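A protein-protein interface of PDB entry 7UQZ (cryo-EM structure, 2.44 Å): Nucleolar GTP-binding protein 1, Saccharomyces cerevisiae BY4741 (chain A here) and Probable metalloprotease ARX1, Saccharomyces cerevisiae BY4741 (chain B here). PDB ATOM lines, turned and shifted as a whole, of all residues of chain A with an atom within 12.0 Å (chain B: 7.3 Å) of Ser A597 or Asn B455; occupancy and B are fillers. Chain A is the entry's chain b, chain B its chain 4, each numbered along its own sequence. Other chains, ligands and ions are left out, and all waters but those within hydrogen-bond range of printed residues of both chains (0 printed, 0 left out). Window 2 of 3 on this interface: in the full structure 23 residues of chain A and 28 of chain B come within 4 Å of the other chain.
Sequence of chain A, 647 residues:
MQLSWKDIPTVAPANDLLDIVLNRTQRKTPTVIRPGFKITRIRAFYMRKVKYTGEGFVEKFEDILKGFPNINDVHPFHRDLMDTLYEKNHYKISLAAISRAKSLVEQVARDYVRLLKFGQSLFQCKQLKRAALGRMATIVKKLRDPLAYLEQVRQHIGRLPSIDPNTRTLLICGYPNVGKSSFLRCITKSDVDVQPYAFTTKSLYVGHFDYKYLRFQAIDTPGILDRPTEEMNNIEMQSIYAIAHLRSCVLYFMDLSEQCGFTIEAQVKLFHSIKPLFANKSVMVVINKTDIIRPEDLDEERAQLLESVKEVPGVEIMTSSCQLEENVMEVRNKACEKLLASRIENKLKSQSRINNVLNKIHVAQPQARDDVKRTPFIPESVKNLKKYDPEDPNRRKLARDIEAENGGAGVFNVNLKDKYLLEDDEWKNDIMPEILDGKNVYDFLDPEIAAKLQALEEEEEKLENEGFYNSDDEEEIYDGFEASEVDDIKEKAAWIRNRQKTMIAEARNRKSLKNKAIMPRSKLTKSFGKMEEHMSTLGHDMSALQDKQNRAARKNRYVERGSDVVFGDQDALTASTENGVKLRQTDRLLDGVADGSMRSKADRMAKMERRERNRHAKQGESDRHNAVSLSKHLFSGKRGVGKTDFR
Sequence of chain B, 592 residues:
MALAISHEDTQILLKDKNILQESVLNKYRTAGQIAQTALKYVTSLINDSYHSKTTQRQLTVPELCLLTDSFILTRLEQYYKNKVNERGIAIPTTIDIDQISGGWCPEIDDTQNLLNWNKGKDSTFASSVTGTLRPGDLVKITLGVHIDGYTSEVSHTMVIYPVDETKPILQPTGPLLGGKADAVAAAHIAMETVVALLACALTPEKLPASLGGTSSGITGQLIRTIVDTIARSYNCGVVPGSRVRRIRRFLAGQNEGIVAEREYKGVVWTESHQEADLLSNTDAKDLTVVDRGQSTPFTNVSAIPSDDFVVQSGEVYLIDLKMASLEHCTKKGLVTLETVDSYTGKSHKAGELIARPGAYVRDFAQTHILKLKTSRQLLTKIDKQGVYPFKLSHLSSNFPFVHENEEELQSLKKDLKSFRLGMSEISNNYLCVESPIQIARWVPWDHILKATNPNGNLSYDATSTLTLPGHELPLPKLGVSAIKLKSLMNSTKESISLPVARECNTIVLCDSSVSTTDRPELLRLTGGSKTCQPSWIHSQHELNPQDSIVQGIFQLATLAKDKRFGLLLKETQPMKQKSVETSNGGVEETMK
The backbone carbonyl oxygen (O) of Ala A594 sits at hydrogen-bond distance from the backbone NH (N) of Ala B462. ND2 of Asn B455 sits at hydrogen-bond distance from OD2 of Asp A595. The backbone carbonyl oxygen (O) of Tyr B460 is in hydrogen-bond range of the backbone NH (N) of Gly A596, at 3.3 Å.
The side-chain carboxylate (OE2) of Glu A578 is in salt-bridge range of the guanidinium group (NH1) of Arg A599 (3.0 Å). O of Leu A590 lies within hydrogen-bond range of NH2 of Arg A599. The backbone carbonyl oxygen (O) of Val A593 is in hydrogen-bond range of the guanidinium group (NE) of Arg A599. The backbone carbonyl oxygen of Gly A596 sits at hydrogen-bond distance from the side-chain hydroxyl of Ser A600 (3.3 Å). O of Ser A597 is in hydrogen-bond range of OG of Ser A600, 2.6 Å away. The side-chain sulfur (SD) of Met A598 lies close to the side-chain amino group (NZ) of Lys A601.
Among the printed residues, pairs that only touch across the chains: Asp A595 with Tyr B460 (3.3 Å), Gly A596 with Ala B462 (3.5 Å), Ser A597 with Leu B458 (3.6 Å), Ser A597 with Asn B455 (3.8 Å), Arg A599 with Ala B462 (3.8 Å) and Met A598 with Asn B455 (3.9 Å).
Ser A597 touches two residues of chain B. Of the printed residues of chain A, Asn B455 touches Asp A595 (3.1 Å), Ser A597 (3.8 Å) and Met A598 (3.9 Å). Gly A596 touches two residues of chain B. Pro B454 touches none of the printed residues of chain A. No residue of chain A comes within 4 Å of Asn B457. Of chain A, only Ser A597 (3.6 Å) comes within 4 Å of Leu B458. Ser B459 touches none of the printed residues of chain A. Of chain A, only Asp A595 (3.3 Å) and Gly A596 (3.3 Å) come within 4 Å of Tyr B460. Printed residues of chain A within 4 Å of Ala B462: Ala A594 (3.3 Å), Gly A596 (3.5 Å) and Arg A599 (3.8 Å). Printed residues of chain B within 4 Å of Met A598: Asn B455. Glu A578 touches none of the printed residues of chain B. The nearest residue of chain B that does not touch Ser A597 is Tyr B460 (4.1 Å). The nearest residue of chain A that does not touch Asn B455 is Lys A601 (5.5 Å).
Of the 18 printed residues of chain A, 6 touch a printed residue of chain B. Hydrophobic or aromatic side chains of chain A within 4 Å of the printed part of chain B: Met A598. Hydrophobic or aromatic side chains of chain B within 4 Å of the printed part of chain A: Leu B458, Tyr B460 and Ala B462. Among the printed residues, 9 pairs touch across the chains. Among the printed residues, no Asp or Glu carboxylate lies within 4 Å of a Lys or Arg side-chain nitrogen of the other chain.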
ATOM      1  N   GLU A 578      16.360  -7.689  10.261  1.00  0.00           N
ATOM      2  CA  GLU A 578      14.954  -7.356  10.456  1.00  0.00           C
ATOM      3  C   GLU A 578      14.653  -6.869  11.867  1.00  0.00           C
ATOM      4  O   GLU A 578      13.747  -6.047  12.043  1.00  0.00           O
ATOM      5  CB  GLU A 578      14.071  -8.565  10.141  1.00  0.00           C
ATOM      6  CG  GLU A 578      14.127  -9.039   8.697  1.00  0.00           C
ATOM      7  CD  GLU A 578      15.219 -10.068   8.454  1.00  0.00           C
ATOM      8  OE1 GLU A 578      16.160 -10.152   9.272  1.00  0.00           O
ATOM      9  OE2 GLU A 578      15.130 -10.798   7.442  1.00  0.00           O
ATOM     10  N   LEU A 590      13.487 -15.550  13.837  1.00  0.00           N
ATOM     11  CA  LEU A 590      13.842 -15.804  12.447  1.00  0.00           C
ATOM     12  C   LEU A 590      15.022 -16.743  12.236  1.00  0.00           C
ATOM     13  O   LEU A 590      15.424 -16.940  11.084  1.00  0.00           O
ATOM     14  CB  LEU A 590      14.140 -14.477  11.733  1.00  0.00           C
ATOM     15  CG  LEU A 590      13.044 -13.414  11.743  1.00  0.00           C
ATOM     16  CD1 LEU A 590      13.507 -12.165  11.011  1.00  0.00           C
ATOM     17  CD2 LEU A 590      11.761 -13.948  11.132  1.00  0.00           C
ATOM     18  N   GLY A 592      15.218 -19.976  12.561  1.00  0.00           N
ATOM     19  CA  GLY A 592      14.839 -21.227  11.940  1.00  0.00           C
ATOM     20  C   GLY A 592      14.450 -21.146  10.483  1.00  0.00           C
ATOM     21  O   GLY A 592      14.185 -22.179   9.864  1.00  0.00           O
ATOM     22  N   VAL A 593      14.397 -19.946   9.911  1.00  0.00           N
ATOM     23  CA  VAL A 593      14.050 -19.747   8.508  1.00  0.00           C
ATOM     24  C   VAL A 593      15.255 -19.110   7.834  1.00  0.00           C
ATOM     25  O   VAL A 593      15.595 -17.954   8.115  1.00  0.00           O
ATOM     26  CB  VAL A 593      12.797 -18.879   8.339  1.00  0.00           C
ATOM     27  CG1 VAL A 593      12.325 -18.918   6.902  1.00  0.00           C
ATOM     28  CG2 VAL A 593      11.696 -19.342   9.280  1.00  0.00           C
ATOM     29  N   ALA A 594      15.902 -19.862   6.941  1.00  0.00           N
ATOM     30  CA  ALA A 594      17.149 -19.403   6.339  1.00  0.00           C
ATOM     31  C   ALA A 594      16.925 -18.333   5.276  1.00  0.00           C
ATOM     32  O   ALA A 594      17.668 -17.347   5.228  1.00  0.00           O
ATOM     33  CB  ALA A 594      17.911 -20.589   5.747  1.00  0.00           C
ATOM     34  N   ASP A 595      15.923 -18.500   4.418  1.00  0.00           N
ATOM     35  CA  ASP A 595      15.785 -17.652   3.243  1.00  0.00           C
ATOM     36  C   ASP A 595      14.671 -16.624   3.408  1.00  0.00           C
ATOM     37  O   ASP A 595      13.625 -16.896   4.012  1.00  0.00           O
ATOM     38  CB  ASP A 595      15.549 -18.488   1.982  1.00  0.00           C
ATOM     39  CG  ASP A 595      14.391 -19.440   2.118  1.00  0.00           C
ATOM     40  OD1 ASP A 595      14.079 -19.842   3.259  1.00  0.00           O
ATOM     41  OD2 ASP A 595      13.798 -19.790   1.078  1.00  0.00           O
ATOM     42  N   GLY A 596      14.911 -15.436   2.847  1.00  0.00           N
ATOM     43  CA  GLY A 596      14.008 -14.312   3.001  1.00  0.00           C
ATOM     44  C   GLY A 596      12.667 -14.491   2.327  1.00  0.00           C
ATOM     45  O   GLY A 596      11.688 -13.885   2.765  1.00  0.00           O
ATOM     46  N   SER A 597      12.593 -15.317   1.282  1.00  0.00           N
ATOM     47  CA  SER A 597      11.305 -15.594   0.652  1.00  0.00           C
ATOM     48  C   SER A 597      10.375 -16.327   1.614  1.00  0.00           C
ATOM     49  O   SER A 597       9.203 -15.957   1.774  1.00  0.00           O
ATOM     50  CB  SER A 597      11.517 -16.402  -0.626  1.00  0.00           C
ATOM     51  OG  SER A 597      10.307 -16.542  -1.349  1.00  0.00           O
ATOM     52  N   MET A 598      10.889 -17.357   2.287  1.00  0.00           N
ATOM     53  CA  MET A 598      10.087 -18.054   3.284  1.00  0.00           C
ATOM     54  C   MET A 598       9.866 -17.193   4.523  1.00  0.00           C
ATOM     55  O   MET A 598       8.824 -17.315   5.177  1.00  0.00           O
ATOM     56  CB  MET A 598      10.741 -19.385   3.650  1.00  0.00           C
ATOM     57  CG  MET A 598      10.945 -20.319   2.469  1.00  0.00           C
ATOM     58  SD  MET A 598       9.418 -20.974   1.766  1.00  0.00           S
ATOM     59  CE  MET A 598       9.040 -22.276   2.936  1.00  0.00           C
ATOM     60  N   ARG A 599      10.816 -16.308   4.848  1.00  0.00           N
ATOM     61  CA  ARG A 599      10.577 -15.348   5.925  1.00  0.00           C
ATOM     62  C   ARG A 599       9.399 -14.433   5.604  1.00  0.00           C
ATOM     63  O   ARG A 599       8.544 -14.182   6.462  1.00  0.00           O
ATOM     64  CB  ARG A 599      11.834 -14.519   6.191  1.00  0.00           C
ATOM     65  CG  ARG A 599      12.959 -15.287   6.852  1.00  0.00           C
ATOM     66  CD  ARG A 599      14.043 -14.359   7.360  1.00  0.00           C
ATOM     67  NE  ARG A 599      15.123 -15.098   8.000  1.00  0.00           N
ATOM     68  CZ  ARG A 599      16.172 -14.538   8.586  1.00  0.00           C
ATOM     69  NH1 ARG A 599      16.313 -13.225   8.641  1.00  0.00           N
ATOM     70  NH2 ARG A 599      17.101 -15.316   9.132  1.00  0.00           N
ATOM     71  N   SER A 600       9.332 -13.940   4.366  1.00  0.00           N
ATOM     72  CA  SER A 600       8.227 -13.078   3.961  1.00  0.00           C
ATOM     73  C   SER A 600       6.914 -13.847   3.914  1.00  0.00           C
ATOM     74  O   SER A 600       5.861 -13.304   4.266  1.00  0.00           O
ATOM     75  CB  SER A 600       8.525 -12.441   2.603  1.00  0.00           C
ATOM     76  OG  SER A 600       8.589 -13.419   1.582  1.00  0.00           O
ATOM     77  N   LYS A 601       6.955 -15.110   3.481  1.00  0.00           N
ATOM     78  CA  LYS A 601       5.742 -15.921   3.488  1.00  0.00           C
ATOM     79  C   LYS A 601       5.222 -16.129   4.908  1.00  0.00           C
ATOM     80  O   LYS A 601       4.017 -16.001   5.160  1.00  0.00           O
ATOM     81  CB  LYS A 601       5.991 -17.267   2.809  1.00  0.00           C
ATOM     82  CG  LYS A 601       4.778 -18.183   2.844  1.00  0.00           C
ATOM     83  CD  LYS A 601       4.929 -19.378   1.922  1.00  0.00           C
ATOM     84  CE  LYS A 601       5.881 -20.407   2.488  1.00  0.00           C
ATOM     85  NZ  LYS A 601       6.030 -21.566   1.565  1.00  0.00           N
ATOM     86  N   ALA A 602       6.120 -16.430   5.850  1.00  0.00           N
ATOM     87  CA  ALA A 602       5.709 -16.600   7.242  1.00  0.00           C
ATOM     88  C   ALA A 602       5.179 -15.296   7.827  1.00  0.00           C
ATOM     89  O   ALA A 602       4.208 -15.301   8.597  1.00  0.00           O
ATOM     90  CB  ALA A 602       6.878 -17.132   8.070  1.00  0.00           C
ATOM     91  N   ASP A 603       5.805 -14.171   7.472  1.00  0.00           N
ATOM     92  CA  ASP A 603       5.324 -12.872   7.932  1.00  0.00           C
ATOM     93  C   ASP A 603       3.923 -12.583   7.411  1.00  0.00           C
ATOM     94  O   ASP A 603       3.065 -12.088   8.154  1.00  0.00           O
ATOM     95  CB  ASP A 603       6.296 -11.778   7.495  1.00  0.00           C
ATOM     96  CG  ASP A 603       5.838 -10.399   7.908  1.00  0.00           C
ATOM     97  OD1 ASP A 603       5.902 -10.087   9.115  1.00  0.00           O
ATOM     98  OD2 ASP A 603       5.413  -9.624   7.027  1.00  0.00           O
ATOM     99  N   ARG A 604       3.670 -12.889   6.135  1.00  0.00           N
ATOM    100  CA  ARG A 604       2.337 -12.690   5.575  1.00  0.00           C
ATOM    101  C   ARG A 604       1.315 -13.595   6.249  1.00  0.00           C
ATOM    102  O   ARG A 604       0.177 -13.177   6.498  1.00  0.00           O
ATOM    103  CB  ARG A 604       2.353 -12.925   4.063  1.00  0.00           C
ATOM    104  CG  ARG A 604       3.108 -11.865   3.276  1.00  0.00           C
ATOM    105  CD  ARG A 604       2.814 -11.952   1.785  1.00  0.00           C
ATOM    106  NE  ARG A 604       3.197 -13.237   1.214  1.00  0.00           N
ATOM    107  CZ  ARG A 604       4.345 -13.471   0.592  1.00  0.00           C
ATOM    108  NH1 ARG A 604       5.251 -12.519   0.431  1.00  0.00           N
ATOM    109  NH2 ARG A 604       4.590 -14.688   0.120  1.00  0.00           N
ATOM    110  N   MET A 605       1.702 -14.836   6.556  1.00  0.00           N
ATOM    111  CA  MET A 605       0.796 -15.745   7.256  1.00  0.00           C
ATOM    112  C   MET A 605       0.425 -15.202   8.633  1.00  0.00           C
ATOM    113  O   MET A 605      -0.750 -15.212   9.022  1.00  0.00           O
ATOM    114  CB  MET A 605       1.430 -17.131   7.377  1.00  0.00           C
ATOM    115  CG  MET A 605       1.560 -17.879   6.062  1.00  0.00           C
ATOM    116  SD  MET A 605       2.540 -19.385   6.201  1.00  0.00           S
ATOM    117  CE  MET A 605       1.499 -20.370   7.270  1.00  0.00           C
ATOM    118  N   ALA A 606       1.417 -14.707   9.380  1.00  0.00           N
ATOM    119  CA  ALA A 606       1.140 -14.159  10.706  1.00  0.00           C
ATOM    120  C   ALA A 606       0.266 -12.910  10.624  1.00  0.00           C
ATOM    121  O   ALA A 606      -0.659 -12.732  11.432  1.00  0.00           O
ATOM    122  CB  ALA A 606       2.449 -13.853  11.434  1.00  0.00           C
ATOM    123  N   MET A 608      -1.902 -12.144   8.256  1.00  0.00           N
ATOM    124  CA  MET A 608      -3.264 -12.542   7.909  1.00  0.00           C
ATOM    125  C   MET A 608      -3.971 -13.187   9.094  1.00  0.00           C
ATOM    126  O   MET A 608      -5.183 -13.020   9.264  1.00  0.00           O
ATOM    127  CB  MET A 608      -3.254 -13.487   6.710  1.00  0.00           C
ATOM    128  CG  MET A 608      -3.262 -12.776   5.368  1.00  0.00           C
ATOM    129  SD  MET A 608      -3.336 -13.906   3.970  1.00  0.00           S
ATOM    130  CE  MET A 608      -1.751 -14.724   4.115  1.00  0.00           C
ATOM    131  N   THR B 452      14.740 -29.317  -7.765  1.00  0.00           N
ATOM    132  CA  THR B 452      13.525 -28.517  -7.700  1.00  0.00           C
ATOM    133  C   THR B 452      13.717 -27.392  -6.694  1.00  0.00           C
ATOM    134  O   THR B 452      14.246 -27.617  -5.601  1.00  0.00           O
ATOM    135  CB  THR B 452      12.317 -29.370  -7.301  1.00  0.00           C
ATOM    136  OG1 THR B 452      12.555 -29.965  -6.018  1.00  0.00           O
ATOM    137  CG2 THR B 452      12.072 -30.464  -8.325  1.00  0.00           C
ATOM    138  N   ASN B 453      13.295 -26.189  -7.066  1.00  0.00           N
ATOM    139  CA  ASN B 453      13.322 -25.034  -6.170  1.00  0.00           C
ATOM    140  C   ASN B 453      11.951 -24.370  -6.181  1.00  0.00           C
ATOM    141  O   ASN B 453      11.588 -23.723  -7.184  1.00  0.00           O
ATOM    142  CB  ASN B 453      14.416 -24.046  -6.570  1.00  0.00           C
ATOM    143  CG  ASN B 453      14.520 -23.866  -8.067  1.00  0.00           C
ATOM    144  OD1 ASN B 453      14.192 -24.768  -8.836  1.00  0.00           O
ATOM    145  ND2 ASN B 453      14.978 -22.695  -8.489  1.00  0.00           N
ATOM    146  N   PRO B 454      11.160 -24.509  -5.111  1.00  0.00           N
ATOM    147  CA  PRO B 454       9.803 -23.938  -5.119  1.00  0.00           C
ATOM    148  C   PRO B 454       9.762 -22.419  -5.140  1.00  0.00           C
ATOM    149  O   PRO B 454       8.704 -21.854  -5.442  1.00  0.00           O
ATOM    150  CB  PRO B 454       9.181 -24.493  -3.828  1.00  0.00           C
ATOM    151  CG  PRO B 454      10.010 -25.692  -3.485  1.00  0.00           C
ATOM    152  CD  PRO B 454      11.397 -25.353  -3.929  1.00  0.00           C
ATOM    153  N   ASN B 455      10.863 -21.738  -4.827  1.00  0.00           N
ATOM    154  CA  ASN B 455      10.887 -20.280  -4.796  1.00  0.00           C
ATOM    155  C   ASN B 455      11.407 -19.658  -6.083  1.00  0.00           C
ATOM    156  O   ASN B 455      10.913 -18.605  -6.496  1.00  0.00           O
ATOM    157  CB  ASN B 455      11.734 -19.791  -3.618  1.00  0.00           C
ATOM    158  CG  ASN B 455      11.143 -20.174  -2.277  1.00  0.00           C
ATOM    159  OD1 ASN B 455       9.925 -20.199  -2.107  1.00  0.00           O
ATOM    160  ND2 ASN B 455      12.007 -20.475  -1.314  1.00  0.00           N
ATOM    161  N   GLY B 456      12.393 -20.277  -6.728  1.00  0.00           N
ATOM    162  CA  GLY B 456      12.928 -19.752  -7.969  1.00  0.00           C
ATOM    163  C   GLY B 456      13.745 -18.486  -7.801  1.00  0.00           C
ATOM    164  O   GLY B 456      14.726 -18.467  -7.055  1.00  0.00           O
ATOM    165  N   ASN B 457      13.346 -17.420  -8.500  1.00  0.00           N
ATOM    166  CA  ASN B 457      14.072 -16.156  -8.420  1.00  0.00           C
ATOM    167  C   ASN B 457      13.932 -15.497  -7.056  1.00  0.00           C
ATOM    168  O   ASN B 457      14.826 -14.757  -6.634  1.00  0.00           O
ATOM    169  CB  ASN B 457      13.578 -15.196  -9.502  1.00  0.00           C
ATOM    170  CG  ASN B 457      14.102 -15.544 -10.872  1.00  0.00           C
ATOM    171  OD1 ASN B 457      15.205 -16.072 -11.010  1.00  0.00           O
ATOM    172  ND2 ASN B 457      13.315 -15.246 -11.899  1.00  0.00           N
ATOM    173  N   LEU B 458      12.824 -15.750  -6.358  1.00  0.00           N
ATOM    174  CA  LEU B 458      12.516 -15.021  -5.135  1.00  0.00           C
ATOM    175  C   LEU B 458      13.417 -15.407  -3.969  1.00  0.00           C
ATOM    176  O   LEU B 458      13.520 -14.640  -3.007  1.00  0.00           O
ATOM    177  CB  LEU B 458      11.052 -15.244  -4.760  1.00  0.00           C
ATOM    178  CG  LEU B 458      10.023 -14.806  -5.803  1.00  0.00           C
ATOM    179  CD1 LEU B 458       8.661 -15.399  -5.488  1.00  0.00           C
ATOM    180  CD2 LEU B 458       9.947 -13.287  -5.869  1.00  0.00           C
ATOM    181  N   SER B 459      14.070 -16.565  -4.032  1.00  0.00           N
ATOM    182  CA  SER B 459      14.881 -17.027  -2.914  1.00  0.00           C
ATOM    183  C   SER B 459      16.196 -16.260  -2.833  1.00  0.00           C
ATOM    184  O   SER B 459      16.805 -15.924  -3.851  1.00  0.00           O
ATOM    185  CB  SER B 459      15.154 -18.526  -3.043  1.00  0.00           C
ATOM    186  OG  SER B 459      15.678 -18.843  -4.320  1.00  0.00           O
ATOM    187  N   TYR B 460      16.621 -15.972  -1.604  1.00  0.00           N
ATOM    188  CA  TYR B 460      17.924 -15.376  -1.344  1.00  0.00           C
ATOM    189  C   TYR B 460      18.330 -15.725   0.079  1.00  0.00           C
ATOM    190  O   TYR B 460      17.490 -16.043   0.922  1.00  0.00           O
ATOM    191  CB  TYR B 460      17.912 -13.856  -1.551  1.00  0.00           C
ATOM    192  CG  TYR B 460      17.132 -13.079  -0.511  1.00  0.00           C
ATOM    193  CD1 TYR B 460      15.758 -12.921  -0.623  1.00  0.00           C
ATOM    194  CD2 TYR B 460      17.773 -12.492   0.574  1.00  0.00           C
ATOM    195  CE1 TYR B 460      15.041 -12.212   0.318  1.00  0.00           C
ATOM    196  CE2 TYR B 460      17.064 -11.782   1.522  1.00  0.00           C
ATOM    197  CZ  TYR B 460      15.700 -11.644   1.389  1.00  0.00           C
ATOM    198  OH  TYR B 460      14.990 -10.937   2.330  1.00  0.00           O
ATOM    199  N   ASP B 461      19.633 -15.655   0.335  1.00  0.00           N
ATOM    200  CA  ASP B 461      20.172 -15.961   1.655  1.00  0.00           C
ATOM    201  C   ASP B 461      19.952 -14.760   2.567  1.00  0.00           C
ATOM    202  O   ASP B 461      20.614 -13.729   2.419  1.00  0.00           O
ATOM    203  CB  ASP B 461      21.652 -16.317   1.553  1.00  0.00           C
ATOM    204  CG  ASP B 461      22.227 -16.809   2.868  1.00  0.00           C
ATOM    205  OD1 ASP B 461      21.441 -17.130   3.783  1.00  0.00           O
ATOM    206  OD2 ASP B 461      23.469 -16.873   2.986  1.00  0.00           O
ATOM    207  N   ALA B 462      19.019 -14.890   3.510  1.00  0.00           N
ATOM    208  CA  ALA B 462      18.719 -13.810   4.438  1.00  0.00           C
ATOM    209  C   ALA B 462      19.682 -13.747   5.615  1.00  0.00           C
ATOM    210  O   ALA B 462      19.737 -12.717   6.295  1.00  0.00           O
ATOM    211  CB  ALA B 462      17.287 -13.947   4.963  1.00  0.00           C
ATOM    212  N   GLY B 479      16.711 -19.631 -12.945  1.00  0.00           N
ATOM    213  CA  GLY B 479      16.120 -19.143 -11.711  1.00  0.00           C
ATOM    214  C   GLY B 479      16.626 -19.828 -10.459  1.00  0.00           C
ATOM    215  O   GLY B 479      15.835 -20.109  -9.551  1.00  0.00           O
ATOM    216  N   SER B 481      19.142 -19.484  -7.254  1.00  0.00           N
ATOM    217  CA  SER B 481      19.854 -18.480  -6.484  1.00  0.00           C
ATOM    218  C   SER B 481      21.110 -19.078  -5.849  1.00  0.00           C
ATOM    219  O   SER B 481      21.411 -20.264  -5.995  1.00  0.00           O
ATOM    220  CB  SER B 481      18.933 -17.877  -5.425  1.00  0.00           C
ATOM    221  OG  SER B 481      18.454 -18.878  -4.547  1.00  0.00           O
